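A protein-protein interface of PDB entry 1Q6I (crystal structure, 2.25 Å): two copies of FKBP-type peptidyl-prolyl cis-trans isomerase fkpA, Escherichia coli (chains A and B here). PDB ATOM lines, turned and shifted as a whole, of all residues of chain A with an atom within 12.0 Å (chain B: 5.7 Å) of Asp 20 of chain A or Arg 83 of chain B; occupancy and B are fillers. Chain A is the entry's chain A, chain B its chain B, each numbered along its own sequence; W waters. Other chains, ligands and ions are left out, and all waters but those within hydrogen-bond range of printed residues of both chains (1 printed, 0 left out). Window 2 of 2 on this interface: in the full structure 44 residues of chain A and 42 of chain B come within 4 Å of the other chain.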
ATOM      1  N   ALA A  15      -3.925   1.565  28.700  1.00  0.00           N
ATOM      2  CA  ALA A  15      -3.260   0.582  27.799  1.00  0.00           C
ATOM      3  C   ALA A  15      -2.783   1.149  26.476  1.00  0.00           C
ATOM      4  O   ALA A  15      -2.732   0.431  25.480  1.00  0.00           O
ATOM      5  CB  ALA A  15      -4.191  -0.549  27.528  1.00  0.00           C
ATOM      6  N   PHE A  16      -2.462   2.430  26.420  1.00  0.00           N
ATOM      7  CA  PHE A  16      -1.933   2.975  25.182  1.00  0.00           C
ATOM      8  C   PHE A  16      -0.469   2.633  24.917  1.00  0.00           C
ATOM      9  O   PHE A  16       0.403   2.812  25.778  1.00  0.00           O
ATOM     10  CB  PHE A  16      -2.166   4.466  25.158  1.00  0.00           C
ATOM     11  CG  PHE A  16      -3.586   4.817  25.374  1.00  0.00           C
ATOM     12  CD1 PHE A  16      -4.512   4.623  24.364  1.00  0.00           C
ATOM     13  CD2 PHE A  16      -4.018   5.265  26.599  1.00  0.00           C
ATOM     14  CE1 PHE A  16      -5.816   4.910  24.557  1.00  0.00           C
ATOM     15  CE2 PHE A  16      -5.333   5.549  26.792  1.00  0.00           C
ATOM     16  CZ  PHE A  16      -6.234   5.363  25.777  1.00  0.00           C
ATOM     17  N   LYS A  17      -0.203   2.192  23.690  1.00  0.00           N
ATOM     18  CA  LYS A  17       1.109   1.724  23.328  1.00  0.00           C
ATOM     19  C   LYS A  17       1.973   2.791  22.682  1.00  0.00           C
ATOM     20  O   LYS A  17       3.182   2.747  22.786  1.00  0.00           O
ATOM     21  CB  LYS A  17       0.992   0.538  22.387  1.00  0.00           C
ATOM     22  CG  LYS A  17      -0.050  -0.495  22.814  1.00  0.00           C
ATOM     23  CD  LYS A  17       0.588  -1.675  23.504  1.00  0.00           C
ATOM     24  CE  LYS A  17      -0.457  -2.645  24.013  1.00  0.00           C
ATOM     25  NZ  LYS A  17      -1.390  -1.983  24.978  1.00  0.00           N
ATOM     26  N   ASN A  18       1.354   3.772  22.056  1.00  0.00           N
ATOM     27  CA  ASN A  18       2.110   4.748  21.310  1.00  0.00           C
ATOM     28  C   ASN A  18       1.356   6.028  21.148  1.00  0.00           C
ATOM     29  O   ASN A  18       0.123   6.054  21.283  1.00  0.00           O
ATOM     30  CB  ASN A  18       2.372   4.219  19.905  1.00  0.00           C
ATOM     31  CG  ASN A  18       1.086   3.911  19.163  1.00  0.00           C
ATOM     32  OD1 ASN A  18       0.365   4.813  18.737  1.00  0.00           O
ATOM     33  ND2 ASN A  18       0.779   2.622  19.029  1.00  0.00           N
ATOM     34  N   ASP A  19       2.115   7.052  20.765  1.00  0.00           N
ATOM     35  CA  ASP A  19       1.596   8.406  20.587  1.00  0.00           C
ATOM     36  C   ASP A  19       0.444   8.472  19.607  1.00  0.00           C
ATOM     37  O   ASP A  19      -0.578   9.084  19.903  1.00  0.00           O
ATOM     38  CB  ASP A  19       2.696   9.401  20.167  1.00  0.00           C
ATOM     39  CG  ASP A  19       2.293  10.832  20.444  1.00  0.00           C
ATOM     40  OD1 ASP A  19       1.803  11.074  21.573  1.00  0.00           O
ATOM     41  OD2 ASP A  19       2.368  11.769  19.612  1.00  0.00           O
ATOM     42  N   ASP A  20       0.579   7.860  18.443  1.00  0.00           N
ATOM     43  CA  ASP A  20      -0.532   7.897  17.512  1.00  0.00           C
ATOM     44  C   ASP A  20      -1.796   7.339  18.167  1.00  0.00           C
ATOM     45  O   ASP A  20      -2.899   7.739  17.834  1.00  0.00           O
ATOM     46  CB  ASP A  20      -0.177   7.200  16.186  1.00  0.00           C
ATOM     47  CG  ASP A  20       0.753   8.077  15.303  1.00  0.00           C
ATOM     48  OD1 ASP A  20       0.706   9.330  15.464  1.00  0.00           O
ATOM     49  OD2 ASP A  20       1.559   7.609  14.454  1.00  0.00           O
ATOM     50  N   GLN A  21      -1.639   6.445  19.127  1.00  0.00           N
ATOM     51  CA  GLN A  21      -2.806   5.901  19.819  1.00  0.00           C
ATOM     52  C   GLN A  21      -3.254   6.818  20.982  1.00  0.00           C
ATOM     53  O   GLN A  21      -4.402   7.264  21.025  1.00  0.00           O
ATOM     54  CB  GLN A  21      -2.559   4.461  20.257  1.00  0.00           C
ATOM     55  CG  GLN A  21      -2.941   3.484  19.162  1.00  0.00           C
ATOM     56  CD  GLN A  21      -2.240   2.135  19.264  1.00  0.00           C
ATOM     57  OE1 GLN A  21      -2.500   1.370  20.183  1.00  0.00           O
ATOM     58  NE2 GLN A  21      -1.358   1.839  18.305  1.00  0.00           N
ATOM     59  N   LYS A  22      -2.319   7.156  21.857  1.00  0.00           N
ATOM     60  CA  LYS A  22      -2.614   7.965  23.025  1.00  0.00           C
ATOM     61  C   LYS A  22      -3.044   9.387  22.713  1.00  0.00           C
ATOM     62  O   LYS A  22      -3.996   9.885  23.314  1.00  0.00           O
ATOM     63  CB  LYS A  22      -1.411   7.979  23.945  1.00  0.00           C
ATOM     64  CG  LYS A  22      -1.668   8.611  25.272  1.00  0.00           C
ATOM     65  CD  LYS A  22      -0.694   8.106  26.310  1.00  0.00           C
ATOM     66  CE  LYS A  22      -0.568   9.075  27.448  1.00  0.00           C
ATOM     67  NZ  LYS A  22       0.274   8.504  28.541  1.00  0.00           N
ATOM     68  N   SER A  23      -2.376  10.054  21.778  1.00  0.00           N
ATOM     69  CA  SER A  23      -2.761  11.428  21.465  1.00  0.00           C
ATOM     70  C   SER A  23      -4.100  11.472  20.790  1.00  0.00           C
ATOM     71  O   SER A  23      -4.794  12.466  20.869  1.00  0.00           O
ATOM     72  CB  SER A  23      -1.779  12.122  20.521  1.00  0.00           C
ATOM     73  OG  SER A  23      -0.538  12.293  21.105  1.00  0.00           O
ATOM     74  N   ALA A  24      -4.412  10.434  20.033  1.00  0.00           N
ATOM     75  CA  ALA A  24      -5.680  10.358  19.332  1.00  0.00           C
ATOM     76  C   ALA A  24      -6.823  10.194  20.342  1.00  0.00           C
ATOM     77  O   ALA A  24      -7.891  10.822  20.203  1.00  0.00           O
ATOM     78  CB  ALA A  24      -5.670   9.193  18.377  1.00  0.00           C
ATOM     79  N   TYR A  25      -6.589   9.350  21.336  1.00  0.00           N
ATOM     80  CA  TYR A  25      -7.576   9.116  22.373  1.00  0.00           C
ATOM     81  C   TYR A  25      -7.780  10.419  23.125  1.00  0.00           C
ATOM     82  O   TYR A  25      -8.906  10.869  23.329  1.00  0.00           O
ATOM     83  CB  TYR A  25      -7.148   8.016  23.318  1.00  0.00           C
ATOM     84  CG  TYR A  25      -8.228   7.664  24.319  1.00  0.00           C
ATOM     85  CD1 TYR A  25      -8.352   8.377  25.510  1.00  0.00           C
ATOM     86  CD2 TYR A  25      -9.137   6.634  24.069  1.00  0.00           C
ATOM     87  CE1 TYR A  25      -9.348   8.091  26.406  1.00  0.00           C
ATOM     88  CE2 TYR A  25     -10.143   6.315  24.991  1.00  0.00           C
ATOM     89  CZ  TYR A  25     -10.243   7.052  26.154  1.00  0.00           C
ATOM     90  OH  TYR A  25     -11.205   6.803  27.098  1.00  0.00           O
ATOM     91  N   ALA A  26      -6.666  11.053  23.459  1.00  0.00           N
ATOM     92  CA  ALA A  26      -6.685  12.295  24.188  1.00  0.00           C
ATOM     93  C   ALA A  26      -7.492  13.319  23.431  1.00  0.00           C
ATOM     94  O   ALA A  26      -8.347  13.981  24.011  1.00  0.00           O
ATOM     95  CB  ALA A  26      -5.247  12.813  24.413  1.00  0.00           C
ATOM     96  N   LEU A  27      -7.169  13.484  22.156  1.00  0.00           N
ATOM     97  CA  LEU A  27      -7.843  14.457  21.311  1.00  0.00           C
ATOM     98  C   LEU A  27      -9.365  14.182  21.286  1.00  0.00           C
ATOM     99  O   LEU A  27     -10.198  15.078  21.491  1.00  0.00           O
ATOM    100  CB  LEU A  27      -7.248  14.420  19.893  1.00  0.00           C
ATOM    101  CG  LEU A  27      -7.082  15.774  19.182  1.00  0.00           C
ATOM    102  CD1 LEU A  27      -6.534  15.547  17.753  1.00  0.00           C
ATOM    103  CD2 LEU A  27      -8.367  16.564  19.110  1.00  0.00           C
ATOM    104  N   GLY A  28      -9.719  12.916  21.107  1.00  0.00           N
ATOM    105  CA  GLY A  28     -11.110  12.529  21.140  1.00  0.00           C
ATOM    106  C   GLY A  28     -11.758  12.834  22.479  1.00  0.00           C
ATOM    107  O   GLY A  28     -12.814  13.472  22.527  1.00  0.00           O
ATOM    108  N   ALA A  29     -11.138  12.384  23.571  1.00  0.00           N
ATOM    109  CA  ALA A  29     -11.709  12.620  24.873  1.00  0.00           C
ATOM    110  C   ALA A  29     -11.918  14.104  25.117  1.00  0.00           C
ATOM    111  O   ALA A  29     -12.909  14.517  25.708  1.00  0.00           O
ATOM    112  CB  ALA A  29     -10.855  12.026  25.942  1.00  0.00           C
ATOM    113  N   PHE A  62     -17.887  10.876  10.247  1.00  0.00           N
ATOM    114  CA  PHE A  62     -16.520  10.381  10.283  1.00  0.00           C
ATOM    115  C   PHE A  62     -16.244   9.408   9.167  1.00  0.00           C
ATOM    116  O   PHE A  62     -15.144   9.337   8.654  1.00  0.00           O
ATOM    117  CB  PHE A  62     -16.210   9.708  11.608  1.00  0.00           C
ATOM    118  CG  PHE A  62     -14.770   9.780  11.972  1.00  0.00           C
ATOM    119  CD1 PHE A  62     -14.142  11.007  12.083  1.00  0.00           C
ATOM    120  CD2 PHE A  62     -14.037   8.637  12.164  1.00  0.00           C
ATOM    121  CE1 PHE A  62     -12.828  11.107  12.412  1.00  0.00           C
ATOM    122  CE2 PHE A  62     -12.705   8.729  12.498  1.00  0.00           C
ATOM    123  CZ  PHE A  62     -12.100   9.982  12.630  1.00  0.00           C
ATOM    124  N   GLY B  46       2.537  14.353   7.380  1.00  0.00           N
ATOM    125  CA  GLY B  46       2.835  12.964   7.616  1.00  0.00           C
ATOM    126  C   GLY B  46       2.374  12.498   8.979  1.00  0.00           C
ATOM    127  O   GLY B  46       2.793  11.419   9.396  1.00  0.00           O
ATOM    128  N   ILE B  47       1.545  13.295   9.670  1.00  0.00           N
ATOM    129  CA  ILE B  47       1.018  12.905  10.990  1.00  0.00           C
ATOM    130  C   ILE B  47      -0.329  12.194  10.839  1.00  0.00           C
ATOM    131  O   ILE B  47      -1.311  12.750  10.377  1.00  0.00           O
ATOM    132  CB  ILE B  47       0.914  14.110  11.942  1.00  0.00           C
ATOM    133  CG1 ILE B  47       2.320  14.591  12.377  1.00  0.00           C
ATOM    134  CG2 ILE B  47       0.105  13.729  13.197  1.00  0.00           C
ATOM    135  CD1 ILE B  47       2.275  15.889  13.198  1.00  0.00           C
ATOM    136  N   LYS B  48      -0.340  10.926  11.196  1.00  0.00           N
ATOM    137  CA  LYS B  48      -1.503  10.077  11.045  1.00  0.00           C
ATOM    138  C   LYS B  48      -2.004   9.499  12.376  1.00  0.00           C
ATOM    139  O   LYS B  48      -1.503   8.501  12.860  1.00  0.00           O
ATOM    140  CB  LYS B  48      -1.158   8.955  10.081  1.00  0.00           C
ATOM    141  CG  LYS B  48      -1.370   9.338   8.606  1.00  0.00           C
ATOM    142  CD  LYS B  48      -0.712   8.348   7.650  1.00  0.00           C
ATOM    143  CE  LYS B  48       0.799   8.384   7.785  1.00  0.00           C
ATOM    144  NZ  LYS B  48       1.420   7.416   6.907  1.00  0.00           N
ATOM    145  N   LEU B  49      -3.012  10.121  12.961  1.00  0.00           N
ATOM    146  CA  LEU B  49      -3.599   9.603  14.181  1.00  0.00           C
ATOM    147  C   LEU B  49      -4.471   8.383  13.963  1.00  0.00           C
ATOM    148  O   LEU B  49      -5.111   8.209  12.907  1.00  0.00           O
ATOM    149  CB  LEU B  49      -4.455  10.675  14.816  1.00  0.00           C
ATOM    150  CG  LEU B  49      -3.690  11.831  15.444  1.00  0.00           C
ATOM    151  CD1 LEU B  49      -4.674  12.856  15.994  1.00  0.00           C
ATOM    152  CD2 LEU B  49      -2.818  11.324  16.532  1.00  0.00           C
ATOM    153  N   ASP B  50      -4.488   7.541  14.979  1.00  0.00           N
ATOM    154  CA  ASP B  50      -5.302   6.324  15.013  1.00  0.00           C
ATOM    155  C   ASP B  50      -6.798   6.681  15.138  1.00  0.00           C
ATOM    156  O   ASP B  50      -7.264   7.118  16.189  1.00  0.00           O
ATOM    157  CB  ASP B  50      -4.829   5.497  16.213  1.00  0.00           C
ATOM    158  CG  ASP B  50      -5.533   4.194  16.343  1.00  0.00           C
ATOM    159  OD1 ASP B  50      -6.776   4.181  16.251  1.00  0.00           O
ATOM    160  OD2 ASP B  50      -4.924   3.121  16.557  1.00  0.00           O
ATOM    161  N   GLN B  53      -9.036   5.045  17.759  1.00  0.00           N
ATOM    162  CA  GLN B  53      -8.848   5.623  19.080  1.00  0.00           C
ATOM    163  C   GLN B  53      -9.459   6.983  19.182  1.00  0.00           C
ATOM    164  O   GLN B  53      -9.962   7.346  20.217  1.00  0.00           O
ATOM    165  CB  GLN B  53      -7.380   5.668  19.485  1.00  0.00           C
ATOM    166  CG  GLN B  53      -6.795   4.304  19.734  1.00  0.00           C
ATOM    167  CD  GLN B  53      -7.280   3.658  21.030  1.00  0.00           C
ATOM    168  OE1 GLN B  53      -8.343   3.973  21.546  1.00  0.00           O
ATOM    169  NE2 GLN B  53      -6.477   2.756  21.556  1.00  0.00           N
ATOM    170  N   GLN B  78      -1.068  18.873  24.912  1.00  0.00           N
ATOM    171  CA  GLN B  78       0.002  19.843  24.920  1.00  0.00           C
ATOM    172  C   GLN B  78       1.208  19.348  24.105  1.00  0.00           C
ATOM    173  O   GLN B  78       1.720  20.053  23.256  1.00  0.00           O
ATOM    174  CB  GLN B  78       0.392  20.099  26.378  1.00  0.00           C
ATOM    175  CG  GLN B  78       1.207  21.340  26.608  1.00  0.00           C
ATOM    176  CD  GLN B  78       1.644  21.439  28.065  1.00  0.00           C
ATOM    177  OE1 GLN B  78       0.861  21.132  28.975  1.00  0.00           O
ATOM    178  NE2 GLN B  78       2.890  21.862  28.290  1.00  0.00           N
ATOM    179  N   ALA B  79       1.654  18.129  24.346  1.00  0.00           N
ATOM    180  CA  ALA B  79       2.804  17.625  23.619  1.00  0.00           C
ATOM    181  C   ALA B  79       2.443  17.388  22.139  1.00  0.00           C
ATOM    182  O   ALA B  79       3.257  17.668  21.268  1.00  0.00           O
ATOM    183  CB  ALA B  79       3.337  16.372  24.243  1.00  0.00           C
ATOM    184  N   PHE B  80       1.216  16.918  21.870  1.00  0.00           N
ATOM    185  CA  PHE B  80       0.817  16.643  20.493  1.00  0.00           C
ATOM    186  C   PHE B  80       0.739  17.918  19.656  1.00  0.00           C
ATOM    187  O   PHE B  80       1.200  17.951  18.520  1.00  0.00           O
ATOM    188  CB  PHE B  80      -0.505  15.914  20.407  1.00  0.00           C
ATOM    189  CG  PHE B  80      -0.952  15.680  19.003  1.00  0.00           C
ATOM    190  CD1 PHE B  80      -0.261  14.811  18.195  1.00  0.00           C
ATOM    191  CD2 PHE B  80      -2.022  16.371  18.478  1.00  0.00           C
ATOM    192  CE1 PHE B  80      -0.637  14.594  16.937  1.00  0.00           C
ATOM    193  CE2 PHE B  80      -2.389  16.174  17.184  1.00  0.00           C
ATOM    194  CZ  PHE B  80      -1.706  15.272  16.410  1.00  0.00           C
ATOM    195  N   GLU B  81       0.178  18.973  20.228  1.00  0.00           N
ATOM    196  CA  GLU B  81       0.072  20.231  19.509  1.00  0.00           C
ATOM    197  C   GLU B  81       1.437  20.925  19.344  1.00  0.00           C
ATOM    198  O   GLU B  81       1.649  21.704  18.391  1.00  0.00           O
ATOM    199  CB  GLU B  81      -0.995  21.124  20.146  1.00  0.00           C
ATOM    200  CG  GLU B  81      -2.406  20.507  20.098  1.00  0.00           C
ATOM    201  CD  GLU B  81      -2.979  20.328  18.679  1.00  0.00           C
ATOM    202  OE1 GLU B  81      -2.234  20.488  17.679  1.00  0.00           O
ATOM    203  OE2 GLU B  81      -4.193  20.022  18.548  1.00  0.00           O
ATOM    204  N   ALA B  82       2.386  20.616  20.226  1.00  0.00           N
ATOM    205  CA  ALA B  82       3.740  21.133  20.031  1.00  0.00           C
ATOM    206  C   ALA B  82       4.350  20.406  18.801  1.00  0.00           C
ATOM    207  O   ALA B  82       5.028  21.019  17.981  1.00  0.00           O
ATOM    208  CB  ALA B  82       4.594  20.930  21.286  1.00  0.00           C
ATOM    209  N   ARG B  83       4.093  19.104  18.688  1.00  0.00           N
ATOM    210  CA  ARG B  83       4.537  18.276  17.555  1.00  0.00           C
ATOM    211  C   ARG B  83       3.967  18.825  16.240  1.00  0.00           C
ATOM    212  O   ARG B  83       4.690  19.066  15.298  1.00  0.00           O
ATOM    213  CB  ARG B  83       4.095  16.821  17.802  1.00  0.00           C
ATOM    214  CG  ARG B  83       4.227  15.765  16.654  1.00  0.00           C
ATOM    215  CD  ARG B  83       3.787  14.318  17.109  1.00  0.00           C
ATOM    216  NE  ARG B  83       3.658  13.348  16.013  1.00  0.00           N
ATOM    217  CZ  ARG B  83       2.858  12.269  16.024  1.00  0.00           C
ATOM    218  NH1 ARG B  83       2.071  11.985  17.055  1.00  0.00           N
ATOM    219  NH2 ARG B  83       2.835  11.454  14.972  1.00  0.00           N
ATOM    220  N   VAL B  84       2.668  19.063  16.201  1.00  0.00           N
ATOM    221  CA  VAL B  84       2.019  19.561  15.005  1.00  0.00           C
ATOM    222  C   VAL B  84       2.587  20.932  14.613  1.00  0.00           C
ATOM    223  O   VAL B  84       2.986  21.147  13.476  1.00  0.00           O
ATOM    224  CB  VAL B  84       0.493  19.650  15.195  1.00  0.00           C
ATOM    225  CG1 VAL B  84      -0.168  20.273  14.005  1.00  0.00           C
ATOM    226  CG2 VAL B  84      -0.088  18.276  15.449  1.00  0.00           C
ATOM    227  N   LYS B  85       2.651  21.851  15.551  1.00  0.00           N
ATOM    228  CA  LYS B  85       3.130  23.154  15.212  1.00  0.00           C
ATOM    229  C   LYS B  85       4.597  23.091  14.793  1.00  0.00           C
ATOM    230  O   LYS B  85       4.997  23.728  13.823  1.00  0.00           O
ATOM    231  CB  LYS B  85       2.900  24.121  16.363  1.00  0.00           C
ATOM    232  CG  LYS B  85       1.487  24.606  16.395  1.00  0.00           C
ATOM    233  CD  LYS B  85       1.088  25.090  17.776  1.00  0.00           C
ATOM    234  CE  LYS B  85      -0.403  25.464  17.826  1.00  0.00           C
ATOM    235  NZ  LYS B  85      -0.756  26.353  18.976  1.00  0.00           N
ATOM    236  N   SER B  86       5.388  22.295  15.495  1.00  0.00           N
ATOM    237  CA  SER B  86       6.776  22.211  15.154  1.00  0.00           C
ATOM    238  C   SER B  86       6.950  21.519  13.803  1.00  0.00           C
ATOM    239  O   SER B  86       7.823  21.894  13.019  1.00  0.00           O
ATOM    240  CB  SER B  86       7.557  21.509  16.240  1.00  0.00           C
ATOM    241  OG  SER B  86       8.645  20.856  15.662  1.00  0.00           O
ATOM    242  N   SER B  87       6.113  20.531  13.492  1.00  0.00           N
ATOM    243  CA  SER B  87       6.204  19.936  12.173  1.00  0.00           C
ATOM    244  C   SER B  87       5.715  20.907  11.042  1.00  0.00           C
ATOM    245  O   SER B  87       6.272  20.939   9.943  1.00  0.00           O
ATOM    246  CB  SER B  87       5.461  18.617  12.134  1.00  0.00           C
ATOM    247  OG  SER B  87       5.388  18.125  10.795  1.00  0.00           O
ATOM    248  N   ALA B  88       4.682  21.688  11.320  1.00  0.00           N
ATOM    249  CA  ALA B  88       4.122  22.590  10.315  1.00  0.00           C
ATOM    250  C   ALA B  88       5.090  23.743  10.030  1.00  0.00           C
ATOM    251  O   ALA B  88       5.227  24.188   8.924  1.00  0.00           O
ATOM    252  CB  ALA B  88       2.817  23.123  10.747  1.00  0.00           C
HETATM  253  O   HOH W   1       1.975   9.119  12.319  1.00  0.00           O
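The side-chain amide oxygen (OD1) of Asn 18 of chain A is in hydrogen-bond range of the backbone NH (N) of Asp 20 of chain A, at 3.1 Å.
The side-chain carboxylate (OD1) of Asp 19 of chain A sits at hydrogen-bond distance from the side-chain hydroxyl (OG) of Ser 23 of chain A.
N of Gln 21 of chain A is in hydrogen-bond range of OD1 of Asn 18 of chain A (2.6 Å).
The side-chain carboxylate (OD1) of Asp 50 of chain B lies within hydrogen-bond range of the backbone NH (N) of Gln 53 of chain B (2.9 Å).
Printed residues of chain B within 4 Å of Phe 16 of chain A: Gln 53 (3.8 Å).
Asp 20 of chain A touches just these residues of chain B: Lys 48 (3.4 Å), Leu 49 (3.8 Å), Asp 50 (3.3 Å) and Arg 83 (3.0 Å).
Printed residues of chain B within 4 Å of Gln 21 of chain A: Asp 50 (3.3 Å) and Gln 53 (3.7 Å).
Printed residues of chain B within 4 Å of Ser 23 of chain A: Phe 80 (3.7 Å).
Printed residues of chain B within 4 Å of Tyr 25 of chain A: Gln 53.
Of the printed residues of chain B, Leu 27 of chain A touches Leu 49 (3.7 Å).
Ile 47 of chain B touches none of the printed residues of chain A.
Of chain A, only Asp 20 (3.4 Å) comes within 4 Å of Lys 48 of chain B.
Of the printed residues of chain A, Leu 49 of chain B touches Asp 20, Ala 24 and Leu 27.
Gln 53 of chain B touches just these residues of chain A: Phe 16, Gln 21 and Tyr 25.
Of the printed residues of chain A, Phe 80 of chain B touches Ser 23.
No residue of chain A comes within 4 Å of Ala 82 of chain B.
Printed residues of chain A within 4 Å of Arg 83 of chain B: Asp 19 and Asp 20.
Ser 86 of chain B touches none of the printed residues of chain A.
No residue of chain A comes within 4 Å of Ser 87 of chain B.
The nearest printed residue of chain B that does not touch Tyr 25 of chain A is Asp 50 of chain B (5.7 Å).
Gln 53 of chain B touches Phe 16 of chain A.
O of Lys 48 of chain B touches CG of Asp 20 of chain A (3.4 Å).
Asp 20 of chain A touches Leu 49 of chain B.
Asp 50 of chain B touches Gln 21 of chain A.
Gln 21 of chain A touches Gln 53 of chain B.
Ser 23 of chain A touches Phe 80 of chain B.
N of Ala 24 of chain A touches CD2 of Leu 49 of chain B, at 3.9 Å.
Asp 50 of chain B touches Ala 24 of chain A (O to CB, 3.4 Å).
O of Gln 53 of chain B touches CA of Tyr 25 of chain A, 3.7 Å away.
CD1 of Leu 49 of chain B touches CD1 of Leu 27 of chain A (3.7 Å).
No position is printed for both chains.
Water W1 bridges OD2 of Asp 20 of chain A (2.6 Å) and N of Lys 48 of chain B (3.1 Å).
The backbone NH (N) of Asp 50 of chain B sits at hydrogen-bond distance from the backbone carbonyl oxygen (O) of Asp 20 of chain A, at 3.3 Å.
The side-chain carboxylate (OD2) of Asp 19 of chain A is in salt-bridge range of the guanidinium group (NH1) of Arg 83 of chain B (2.6 Å).
OD1 of Asp 20 of chain A lies within salt-bridge range of NH2 of Arg 83 of chain B (3.0 Å).
Printed residues of chain B that touch a printed residue of chain A: Lys 48, Leu 49, Asp 50, Gln 53, Phe 80 and Arg 83.
Of the 16 printed residues of chain A, 8 touch a printed residue of chain B.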
